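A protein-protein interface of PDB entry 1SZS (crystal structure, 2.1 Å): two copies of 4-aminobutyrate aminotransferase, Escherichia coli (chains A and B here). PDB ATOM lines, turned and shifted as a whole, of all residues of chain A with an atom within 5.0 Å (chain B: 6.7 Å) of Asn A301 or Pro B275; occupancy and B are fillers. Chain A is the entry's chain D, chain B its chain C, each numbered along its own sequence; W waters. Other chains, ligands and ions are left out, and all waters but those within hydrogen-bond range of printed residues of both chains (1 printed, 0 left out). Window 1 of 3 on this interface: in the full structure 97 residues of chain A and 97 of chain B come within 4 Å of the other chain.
Hydrophobic or aromatic side chains of chain B within 4 Å of the printed part of chain A: Phe B274, Pro B275 and Tyr B298. Printed residues of chain A that touch a printed residue of chain B: Ser A74, His A75, Thr A109, Pro A275, Leu A276, Tyr A298 and Asn A301. Hydrophobic or aromatic side chains of chain A that line the printed part of chain B: His A75, Pro A275 and Tyr A298.
Water W1 lies within hydrogen-bond range of O of Phe B274 (2.7 Å), N of Gly B273 (2.8 Å) and OH of Tyr A298 (3.3 Å).
The side-chain amide oxygen of Asn A301 lies within hydrogen-bond range of the backbone NH of Ala A304. O of Thr A109 lies close to N of Leu A276. The backbone NH (N) of Ala B304 is in hydrogen-bond range of the side-chain amide oxygen (OD1) of Asn B301, at 3.2 Å. The backbone carbonyl oxygen (O) of Asn A301 lies within hydrogen-bond range of the side-chain sulfur (SG) of Cys A305 (3.4 Å). The backbone NH (N) of Leu B276 sits close to the backbone carbonyl oxygen (O) of Thr B109 (3.3 Å). SG of Cys B305 is in hydrogen-bond range of O of Asn B301 (3.4 Å).
Thr A109 touches its own counterpart, Thr B109. Thr A109 touches Tyr B298, and with the chains exchanged Tyr A298 touches Thr B109. Pro A275 touches Tyr B298, and with the chains exchanged Tyr A298 touches Pro B275. Leu A276 touches Tyr B298, and with the chains exchanged Tyr A298 touches Leu B276.
Of the printed residues of chain B, His A75 touches Gly B273. Printed residues of chain A within 4 Å of Thr B109: Thr A109 (3.5 Å) and Tyr A298 (3.3 Å). Ala B271 touches none of the printed residues of chain A. Pro B275 touches just these residues of chain A: Tyr A298 and Asn A301. Gly B300 touches none of the printed residues of chain A. The nearest residue of chain B that does not touch Asn A301 is Gly B273 (4.2 Å). The nearest printed residue of chain B that does not touch Pro A275 is Pro B275 (4.05 Å).
Ser A74 touches Phe B274 (CB to CZ, 3.6 Å). His A75 touches Gly B273 (CB to O, 3.6 Å). CG2 of Thr A109 touches CG2 of Thr B109 (3.5 Å). CB of Thr A109 touches CG2 of Thr B110, at 3.7 Å. Thr A109 touches Tyr B298. Pro A275 touches Tyr B298 (CA to CE2, 3.6 Å). Pro A275 touches Asn B301. Tyr A298 touches Thr B109. Pro B275 touches Tyr A298 (CA to CE2, 3.7 Å). Asn A301 touches Pro B275.
OH of Tyr B298 sits at hydrogen-bond distance from O of Leu A276 (2.8 Å). The side-chain hydroxyl of Ser A74 is in hydrogen-bond range of the backbone carbonyl oxygen of Gly B273, at 2.6 Å. The backbone carbonyl oxygen (O) of Phe B274 lies within hydrogen-bond range of the side-chain hydroxyl (OH) of Tyr A298, at 3.4 Å. The side-chain hydroxyl of Tyr A298 sits at hydrogen-bond distance from the backbone carbonyl oxygen of Leu B276, 2.6 Å away.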
ATOM      1  N   SER A  74     -19.845   4.157 -16.193  1.00  0.00           N
ATOM      2  CA  SER A  74     -20.093   3.659 -14.846  1.00  0.00           C
ATOM      3  C   SER A  74     -20.376   2.176 -14.799  1.00  0.00           C
ATOM      4  O   SER A  74     -20.221   1.580 -13.744  1.00  0.00           O
ATOM      5  CB  SER A  74     -21.260   4.402 -14.183  1.00  0.00           C
ATOM      6  OG  SER A  74     -22.511   3.906 -14.651  1.00  0.00           O
ATOM      7  N   HIS A  75     -20.766   1.579 -15.921  1.00  0.00           N
ATOM      8  CA  HIS A  75     -21.091   0.156 -15.942  1.00  0.00           C
ATOM      9  C   HIS A  75     -21.173  -0.437 -17.349  1.00  0.00           C
ATOM     10  O   HIS A  75     -21.674   0.209 -18.258  1.00  0.00           O
ATOM     11  CB  HIS A  75     -22.445  -0.059 -15.260  1.00  0.00           C
ATOM     12  CG  HIS A  75     -23.021  -1.433 -15.448  1.00  0.00           C
ATOM     13  ND1 HIS A  75     -22.835  -2.454 -14.537  1.00  0.00           N
ATOM     14  CD2 HIS A  75     -23.771  -1.957 -16.449  1.00  0.00           C
ATOM     15  CE1 HIS A  75     -23.446  -3.545 -14.968  1.00  0.00           C
ATOM     16  NE2 HIS A  75     -24.021  -3.270 -16.125  1.00  0.00           N
ATOM     17  N   TYR A  83     -13.091  -3.914 -18.821  1.00  0.00           N
ATOM     18  CA  TYR A  83     -12.596  -2.551 -18.643  1.00  0.00           C
ATOM     19  C   TYR A  83     -11.385  -2.638 -17.750  1.00  0.00           C
ATOM     20  O   TYR A  83     -11.309  -3.512 -16.878  1.00  0.00           O
ATOM     21  CB  TYR A  83     -13.676  -1.601 -18.085  1.00  0.00           C
ATOM     22  CG  TYR A  83     -14.569  -2.173 -17.011  1.00  0.00           C
ATOM     23  CD1 TYR A  83     -14.181  -2.165 -15.666  1.00  0.00           C
ATOM     24  CD2 TYR A  83     -15.782  -2.769 -17.341  1.00  0.00           C
ATOM     25  CE1 TYR A  83     -14.975  -2.748 -14.686  1.00  0.00           C
ATOM     26  CE2 TYR A  83     -16.585  -3.357 -16.357  1.00  0.00           C
ATOM     27  CZ  TYR A  83     -16.173  -3.349 -15.045  1.00  0.00           C
ATOM     28  OH  TYR A  83     -16.930  -3.994 -14.089  1.00  0.00           O
ATOM     29  N   VAL A 108     -16.504  -8.965  -6.997  1.00  0.00           N
ATOM     30  CA  VAL A 108     -17.958  -9.032  -6.996  1.00  0.00           C
ATOM     31  C   VAL A 108     -18.454  -7.667  -6.432  1.00  0.00           C
ATOM     32  O   VAL A 108     -17.882  -6.630  -6.765  1.00  0.00           O
ATOM     33  CB  VAL A 108     -18.511 -10.262  -6.202  1.00  0.00           C
ATOM     34  CG1 VAL A 108     -18.197 -11.537  -6.989  1.00  0.00           C
ATOM     35  CG2 VAL A 108     -17.915 -10.340  -4.792  1.00  0.00           C
ATOM     36  N   THR A 109     -19.480  -7.641  -5.595  1.00  0.00           N
ATOM     37  CA  THR A 109     -19.951  -6.350  -5.099  1.00  0.00           C
ATOM     38  C   THR A 109     -20.056  -6.269  -3.578  1.00  0.00           C
ATOM     39  O   THR A 109     -19.629  -5.273  -2.999  1.00  0.00           O
ATOM     40  CB  THR A 109     -21.322  -5.973  -5.750  1.00  0.00           C
ATOM     41  OG1 THR A 109     -21.187  -6.005  -7.181  1.00  0.00           O
ATOM     42  CG2 THR A 109     -21.775  -4.556  -5.320  1.00  0.00           C
ATOM     43  N   PRO A 275     -19.359   0.591  -3.307  1.00  0.00           N
ATOM     44  CA  PRO A 275     -19.681  -0.836  -3.384  1.00  0.00           C
ATOM     45  C   PRO A 275     -18.731  -1.724  -4.174  1.00  0.00           C
ATOM     46  O   PRO A 275     -18.770  -1.747  -5.402  1.00  0.00           O
ATOM     47  CB  PRO A 275     -21.104  -0.848  -3.967  1.00  0.00           C
ATOM     48  CG  PRO A 275     -21.615   0.544  -3.711  1.00  0.00           C
ATOM     49  CD  PRO A 275     -20.402   1.384  -3.975  1.00  0.00           C
ATOM     50  N   LEU A 276     -17.911  -2.481  -3.459  1.00  0.00           N
ATOM     51  CA  LEU A 276     -16.960  -3.384  -4.106  1.00  0.00           C
ATOM     52  C   LEU A 276     -16.541  -4.489  -3.151  1.00  0.00           C
ATOM     53  O   LEU A 276     -16.352  -4.241  -1.953  1.00  0.00           O
ATOM     54  CB  LEU A 276     -15.710  -2.612  -4.561  1.00  0.00           C
ATOM     55  CG  LEU A 276     -14.675  -3.468  -5.325  1.00  0.00           C
ATOM     56  CD1 LEU A 276     -15.234  -3.862  -6.670  1.00  0.00           C
ATOM     57  CD2 LEU A 276     -13.379  -2.696  -5.548  1.00  0.00           C
ATOM     58  N   TYR A 298     -23.295  -6.254 -11.364  1.00  0.00           N
ATOM     59  CA  TYR A 298     -22.545  -5.067 -10.963  1.00  0.00           C
ATOM     60  C   TYR A 298     -21.102  -5.355 -10.580  1.00  0.00           C
ATOM     61  O   TYR A 298     -20.343  -4.420 -10.295  1.00  0.00           O
ATOM     62  CB  TYR A 298     -23.219  -4.413  -9.752  1.00  0.00           C
ATOM     63  CG  TYR A 298     -24.637  -3.940  -9.953  1.00  0.00           C
ATOM     64  CD1 TYR A 298     -24.987  -3.146 -11.039  1.00  0.00           C
ATOM     65  CD2 TYR A 298     -25.602  -4.173  -8.967  1.00  0.00           C
ATOM     66  CE1 TYR A 298     -26.266  -2.578 -11.133  1.00  0.00           C
ATOM     67  CE2 TYR A 298     -26.869  -3.617  -9.053  1.00  0.00           C
ATOM     68  CZ  TYR A 298     -27.192  -2.818 -10.127  1.00  0.00           C
ATOM     69  OH  TYR A 298     -28.428  -2.223 -10.151  1.00  0.00           O
ATOM     70  N   ALA A 299     -20.727  -6.630 -10.563  1.00  0.00           N
ATOM     71  CA  ALA A 299     -19.377  -7.043 -10.153  1.00  0.00           C
ATOM     72  C   ALA A 299     -18.234  -6.140 -10.577  1.00  0.00           C
ATOM     73  O   ALA A 299     -18.107  -5.788 -11.753  1.00  0.00           O
ATOM     74  CB  ALA A 299     -19.110  -8.459 -10.642  1.00  0.00           C
ATOM     75  N   GLY A 300     -17.383  -5.782  -9.626  1.00  0.00           N
ATOM     76  CA  GLY A 300     -16.249  -4.943  -9.962  1.00  0.00           C
ATOM     77  C   GLY A 300     -16.679  -3.690 -10.685  1.00  0.00           C
ATOM     78  O   GLY A 300     -16.185  -3.352 -11.772  1.00  0.00           O
ATOM     79  N   ASN A 301     -17.620  -2.998 -10.072  1.00  0.00           N
ATOM     80  CA  ASN A 301     -18.129  -1.751 -10.616  1.00  0.00           C
ATOM     81  C   ASN A 301     -16.958  -0.808 -10.943  1.00  0.00           C
ATOM     82  O   ASN A 301     -16.114  -0.562 -10.069  1.00  0.00           O
ATOM     83  CB  ASN A 301     -19.044  -1.100  -9.577  1.00  0.00           C
ATOM     84  CG  ASN A 301     -19.492   0.277  -9.986  1.00  0.00           C
ATOM     85  OD1 ASN A 301     -18.918   1.300  -9.551  1.00  0.00           O
ATOM     86  ND2 ASN A 301     -20.510   0.323 -10.856  1.00  0.00           N
ATOM     87  N   PRO A 302     -16.902  -0.265 -12.183  1.00  0.00           N
ATOM     88  CA  PRO A 302     -15.848   0.650 -12.638  1.00  0.00           C
ATOM     89  C   PRO A 302     -15.529   1.770 -11.642  1.00  0.00           C
ATOM     90  O   PRO A 302     -14.375   1.959 -11.298  1.00  0.00           O
ATOM     91  CB  PRO A 302     -16.401   1.206 -13.951  1.00  0.00           C
ATOM     92  CG  PRO A 302     -17.223   0.099 -14.453  1.00  0.00           C
ATOM     93  CD  PRO A 302     -17.904  -0.471 -13.243  1.00  0.00           C
ATOM     94  N   ILE A 303     -16.534   2.513 -11.189  1.00  0.00           N
ATOM     95  CA  ILE A 303     -16.271   3.603 -10.241  1.00  0.00           C
ATOM     96  C   ILE A 303     -15.663   3.054  -8.947  1.00  0.00           C
ATOM     97  O   ILE A 303     -14.691   3.597  -8.439  1.00  0.00           O
ATOM     98  CB  ILE A 303     -17.577   4.406  -9.888  1.00  0.00           C
ATOM     99  CG1 ILE A 303     -17.982   5.345 -11.036  1.00  0.00           C
ATOM    100  CG2 ILE A 303     -17.333   5.284  -8.682  1.00  0.00           C
ATOM    101  CD1 ILE A 303     -18.220   4.676 -12.328  1.00  0.00           C
ATOM    102  N   ALA A 304     -16.221   1.977  -8.406  1.00  0.00           N
ATOM    103  CA  ALA A 304     -15.678   1.449  -7.170  1.00  0.00           C
ATOM    104  C   ALA A 304     -14.249   0.891  -7.351  1.00  0.00           C
ATOM    105  O   ALA A 304     -13.439   0.944  -6.416  1.00  0.00           O
ATOM    106  CB  ALA A 304     -16.630   0.387  -6.574  1.00  0.00           C
ATOM    107  N   CYS A 305     -13.936   0.383  -8.538  1.00  0.00           N
ATOM    108  CA  CYS A 305     -12.600  -0.140  -8.808  1.00  0.00           C
ATOM    109  C   CYS A 305     -11.565   0.992  -8.754  1.00  0.00           C
ATOM    110  O   CYS A 305     -10.511   0.841  -8.143  1.00  0.00           O
ATOM    111  CB  CYS A 305     -12.543  -0.808 -10.195  1.00  0.00           C
ATOM    112  SG  CYS A 305     -13.317  -2.441 -10.336  1.00  0.00           S
ATOM    113  N   VAL B 108     -31.071  -3.181  -1.002  1.00  0.00           N
ATOM    114  CA  VAL B 108     -29.832  -3.908  -0.744  1.00  0.00           C
ATOM    115  C   VAL B 108     -28.926  -3.460  -1.890  1.00  0.00           C
ATOM    116  O   VAL B 108     -29.074  -2.323  -2.346  1.00  0.00           O
ATOM    117  CB  VAL B 108     -30.018  -5.461  -0.711  1.00  0.00           C
ATOM    118  CG1 VAL B 108     -30.803  -5.853   0.567  1.00  0.00           C
ATOM    119  CG2 VAL B 108     -30.768  -5.960  -1.947  1.00  0.00           C
ATOM    120  N   THR B 109     -28.034  -4.317  -2.382  1.00  0.00           N
ATOM    121  CA  THR B 109     -27.140  -3.875  -3.446  1.00  0.00           C
ATOM    122  C   THR B 109     -27.216  -4.624  -4.769  1.00  0.00           C
ATOM    123  O   THR B 109     -27.225  -3.973  -5.819  1.00  0.00           O
ATOM    124  CB  THR B 109     -25.696  -3.883  -2.955  1.00  0.00           C
ATOM    125  OG1 THR B 109     -25.614  -3.124  -1.737  1.00  0.00           O
ATOM    126  CG2 THR B 109     -24.759  -3.263  -4.024  1.00  0.00           C
ATOM    127  N   THR B 110     -27.270  -5.956  -4.734  1.00  0.00           N
ATOM    128  CA  THR B 110     -27.327  -6.737  -5.979  1.00  0.00           C
ATOM    129  C   THR B 110     -28.659  -7.484  -6.181  1.00  0.00           C
ATOM    130  O   THR B 110     -29.408  -7.711  -5.232  1.00  0.00           O
ATOM    131  CB  THR B 110     -26.170  -7.793  -6.051  1.00  0.00           C
ATOM    132  OG1 THR B 110     -26.430  -8.853  -5.125  1.00  0.00           O
ATOM    133  CG2 THR B 110     -24.831  -7.149  -5.697  1.00  0.00           C
ATOM    134  N   ALA B 271     -31.102   1.819 -11.262  1.00  0.00           N
ATOM    135  CA  ALA B 271     -30.184   2.942 -11.026  1.00  0.00           C
ATOM    136  C   ALA B 271     -29.308   3.369 -12.206  1.00  0.00           C
ATOM    137  O   ALA B 271     -28.311   4.061 -12.019  1.00  0.00           O
ATOM    138  CB  ALA B 271     -29.319   2.675  -9.810  1.00  0.00           C
ATOM    139  N   GLY B 273     -26.972   2.106 -14.021  1.00  0.00           N
ATOM    140  CA  GLY B 273     -25.547   1.860 -14.079  1.00  0.00           C
ATOM    141  C   GLY B 273     -24.793   2.076 -12.789  1.00  0.00           C
ATOM    142  O   GLY B 273     -23.593   2.316 -12.836  1.00  0.00           O
ATOM    143  N   PHE B 274     -25.490   2.009 -11.651  1.00  0.00           N
ATOM    144  CA  PHE B 274     -24.875   2.157 -10.326  1.00  0.00           C
ATOM    145  C   PHE B 274     -25.408   0.985  -9.472  1.00  0.00           C
ATOM    146  O   PHE B 274     -26.581   0.629  -9.588  1.00  0.00           O
ATOM    147  CB  PHE B 274     -25.212   3.526  -9.731  1.00  0.00           C
ATOM    148  CG  PHE B 274     -24.589   4.665 -10.497  1.00  0.00           C
ATOM    149  CD1 PHE B 274     -25.202   5.161 -11.643  1.00  0.00           C
ATOM    150  CD2 PHE B 274     -23.327   5.143 -10.148  1.00  0.00           C
ATOM    151  CE1 PHE B 274     -24.570   6.106 -12.444  1.00  0.00           C
ATOM    152  CE2 PHE B 274     -22.678   6.099 -10.949  1.00  0.00           C
ATOM    153  CZ  PHE B 274     -23.301   6.572 -12.092  1.00  0.00           C
ATOM    154  N   PRO B 275     -24.563   0.391  -8.607  1.00  0.00           N
ATOM    155  CA  PRO B 275     -24.966  -0.750  -7.777  1.00  0.00           C
ATOM    156  C   PRO B 275     -26.090  -0.531  -6.764  1.00  0.00           C
ATOM    157  O   PRO B 275     -25.874   0.017  -5.681  1.00  0.00           O
ATOM    158  CB  PRO B 275     -23.655  -1.181  -7.092  1.00  0.00           C
ATOM    159  CG  PRO B 275     -22.566  -0.453  -7.850  1.00  0.00           C
ATOM    160  CD  PRO B 275     -23.225   0.847  -8.217  1.00  0.00           C
ATOM    161  N   LEU B 276     -27.283  -0.985  -7.124  1.00  0.00           N
ATOM    162  CA  LEU B 276     -28.432  -0.877  -6.236  1.00  0.00           C
ATOM    163  C   LEU B 276     -29.430  -1.973  -6.597  1.00  0.00           C
ATOM    164  O   LEU B 276     -29.506  -2.395  -7.746  1.00  0.00           O
ATOM    165  CB  LEU B 276     -29.099   0.509  -6.376  1.00  0.00           C
ATOM    166  CG  LEU B 276     -30.344   0.711  -5.484  1.00  0.00           C
ATOM    167  CD1 LEU B 276     -29.925   0.897  -4.037  1.00  0.00           C
ATOM    168  CD2 LEU B 276     -31.122   1.919  -5.931  1.00  0.00           C
ATOM    169  N   ALA B 277     -30.191  -2.419  -5.612  1.00  0.00           N
ATOM    170  CA  ALA B 277     -31.222  -3.430  -5.805  1.00  0.00           C
ATOM    171  C   ALA B 277     -32.174  -3.298  -4.609  1.00  0.00           C
ATOM    172  O   ALA B 277     -31.862  -2.594  -3.645  1.00  0.00           O
ATOM    173  CB  ALA B 277     -30.599  -4.849  -5.832  1.00  0.00           C
ATOM    174  N   TYR B 298     -23.232  -2.218   2.253  1.00  0.00           N
ATOM    175  CA  TYR B 298     -23.415  -1.193   1.217  1.00  0.00           C
ATOM    176  C   TYR B 298     -24.859  -0.924   0.836  1.00  0.00           C
ATOM    177  O   TYR B 298     -25.107  -0.029   0.035  1.00  0.00           O
ATOM    178  CB  TYR B 298     -22.689  -1.590  -0.077  1.00  0.00           C
ATOM    179  CG  TYR B 298     -21.200  -1.836   0.040  1.00  0.00           C
ATOM    180  CD1 TYR B 298     -20.367  -0.912   0.679  1.00  0.00           C
ATOM    181  CD2 TYR B 298     -20.606  -2.921  -0.607  1.00  0.00           C
ATOM    182  CE1 TYR B 298     -18.984  -1.054   0.644  1.00  0.00           C
ATOM    183  CE2 TYR B 298     -19.221  -3.076  -0.631  1.00  0.00           C
ATOM    184  CZ  TYR B 298     -18.421  -2.135  -0.011  1.00  0.00           C
ATOM    185  OH  TYR B 298     -17.054  -2.269  -0.042  1.00  0.00           O
ATOM    186  N   GLY B 300     -28.435   0.016  -0.285  1.00  0.00           N
ATOM    187  CA  GLY B 300     -28.965   1.330  -0.617  1.00  0.00           C
ATOM    188  C   GLY B 300     -27.878   2.395  -0.587  1.00  0.00           C
ATOM    189  O   GLY B 300     -28.020   3.433   0.057  1.00  0.00           O
ATOM    190  N   ASN B 301     -26.775   2.126  -1.271  1.00  0.00           N
ATOM    191  CA  ASN B 301     -25.684   3.072  -1.307  1.00  0.00           C
ATOM    192  C   ASN B 301     -26.186   4.481  -1.717  1.00  0.00           C
ATOM    193  O   ASN B 301     -26.946   4.624  -2.656  1.00  0.00           O
ATOM    194  CB  ASN B 301     -24.624   2.560  -2.275  1.00  0.00           C
ATOM    195  CG  ASN B 301     -23.595   3.595  -2.578  1.00  0.00           C
ATOM    196  OD1 ASN B 301     -23.743   4.371  -3.541  1.00  0.00           O
ATOM    197  ND2 ASN B 301     -22.542   3.649  -1.745  1.00  0.00           N
ATOM    198  N   ALA B 304     -25.984   5.490  -5.522  1.00  0.00           N
ATOM    199  CA  ALA B 304     -26.841   4.701  -6.384  1.00  0.00           C
ATOM    200  C   ALA B 304     -28.307   5.092  -6.119  1.00  0.00           C
ATOM    201  O   ALA B 304     -29.128   5.076  -7.032  1.00  0.00           O
ATOM    202  CB  ALA B 304     -26.604   3.199  -6.137  1.00  0.00           C
ATOM    203  N   CYS B 305     -28.627   5.449  -4.875  1.00  0.00           N
ATOM    204  CA  CYS B 305     -29.979   5.869  -4.548  1.00  0.00           C
ATOM    205  C   CYS B 305     -30.341   7.161  -5.312  1.00  0.00           C
ATOM    206  O   CYS B 305     -31.388   7.217  -5.954  1.00  0.00           O
ATOM    207  CB  CYS B 305     -30.111   6.135  -3.051  1.00  0.00           C
ATOM    208  SG  CYS B 305     -30.312   4.683  -2.040  1.00  0.00           S
HETATM  209  O   HOH W   1     -27.924   0.458 -11.925  1.00  0.00           O
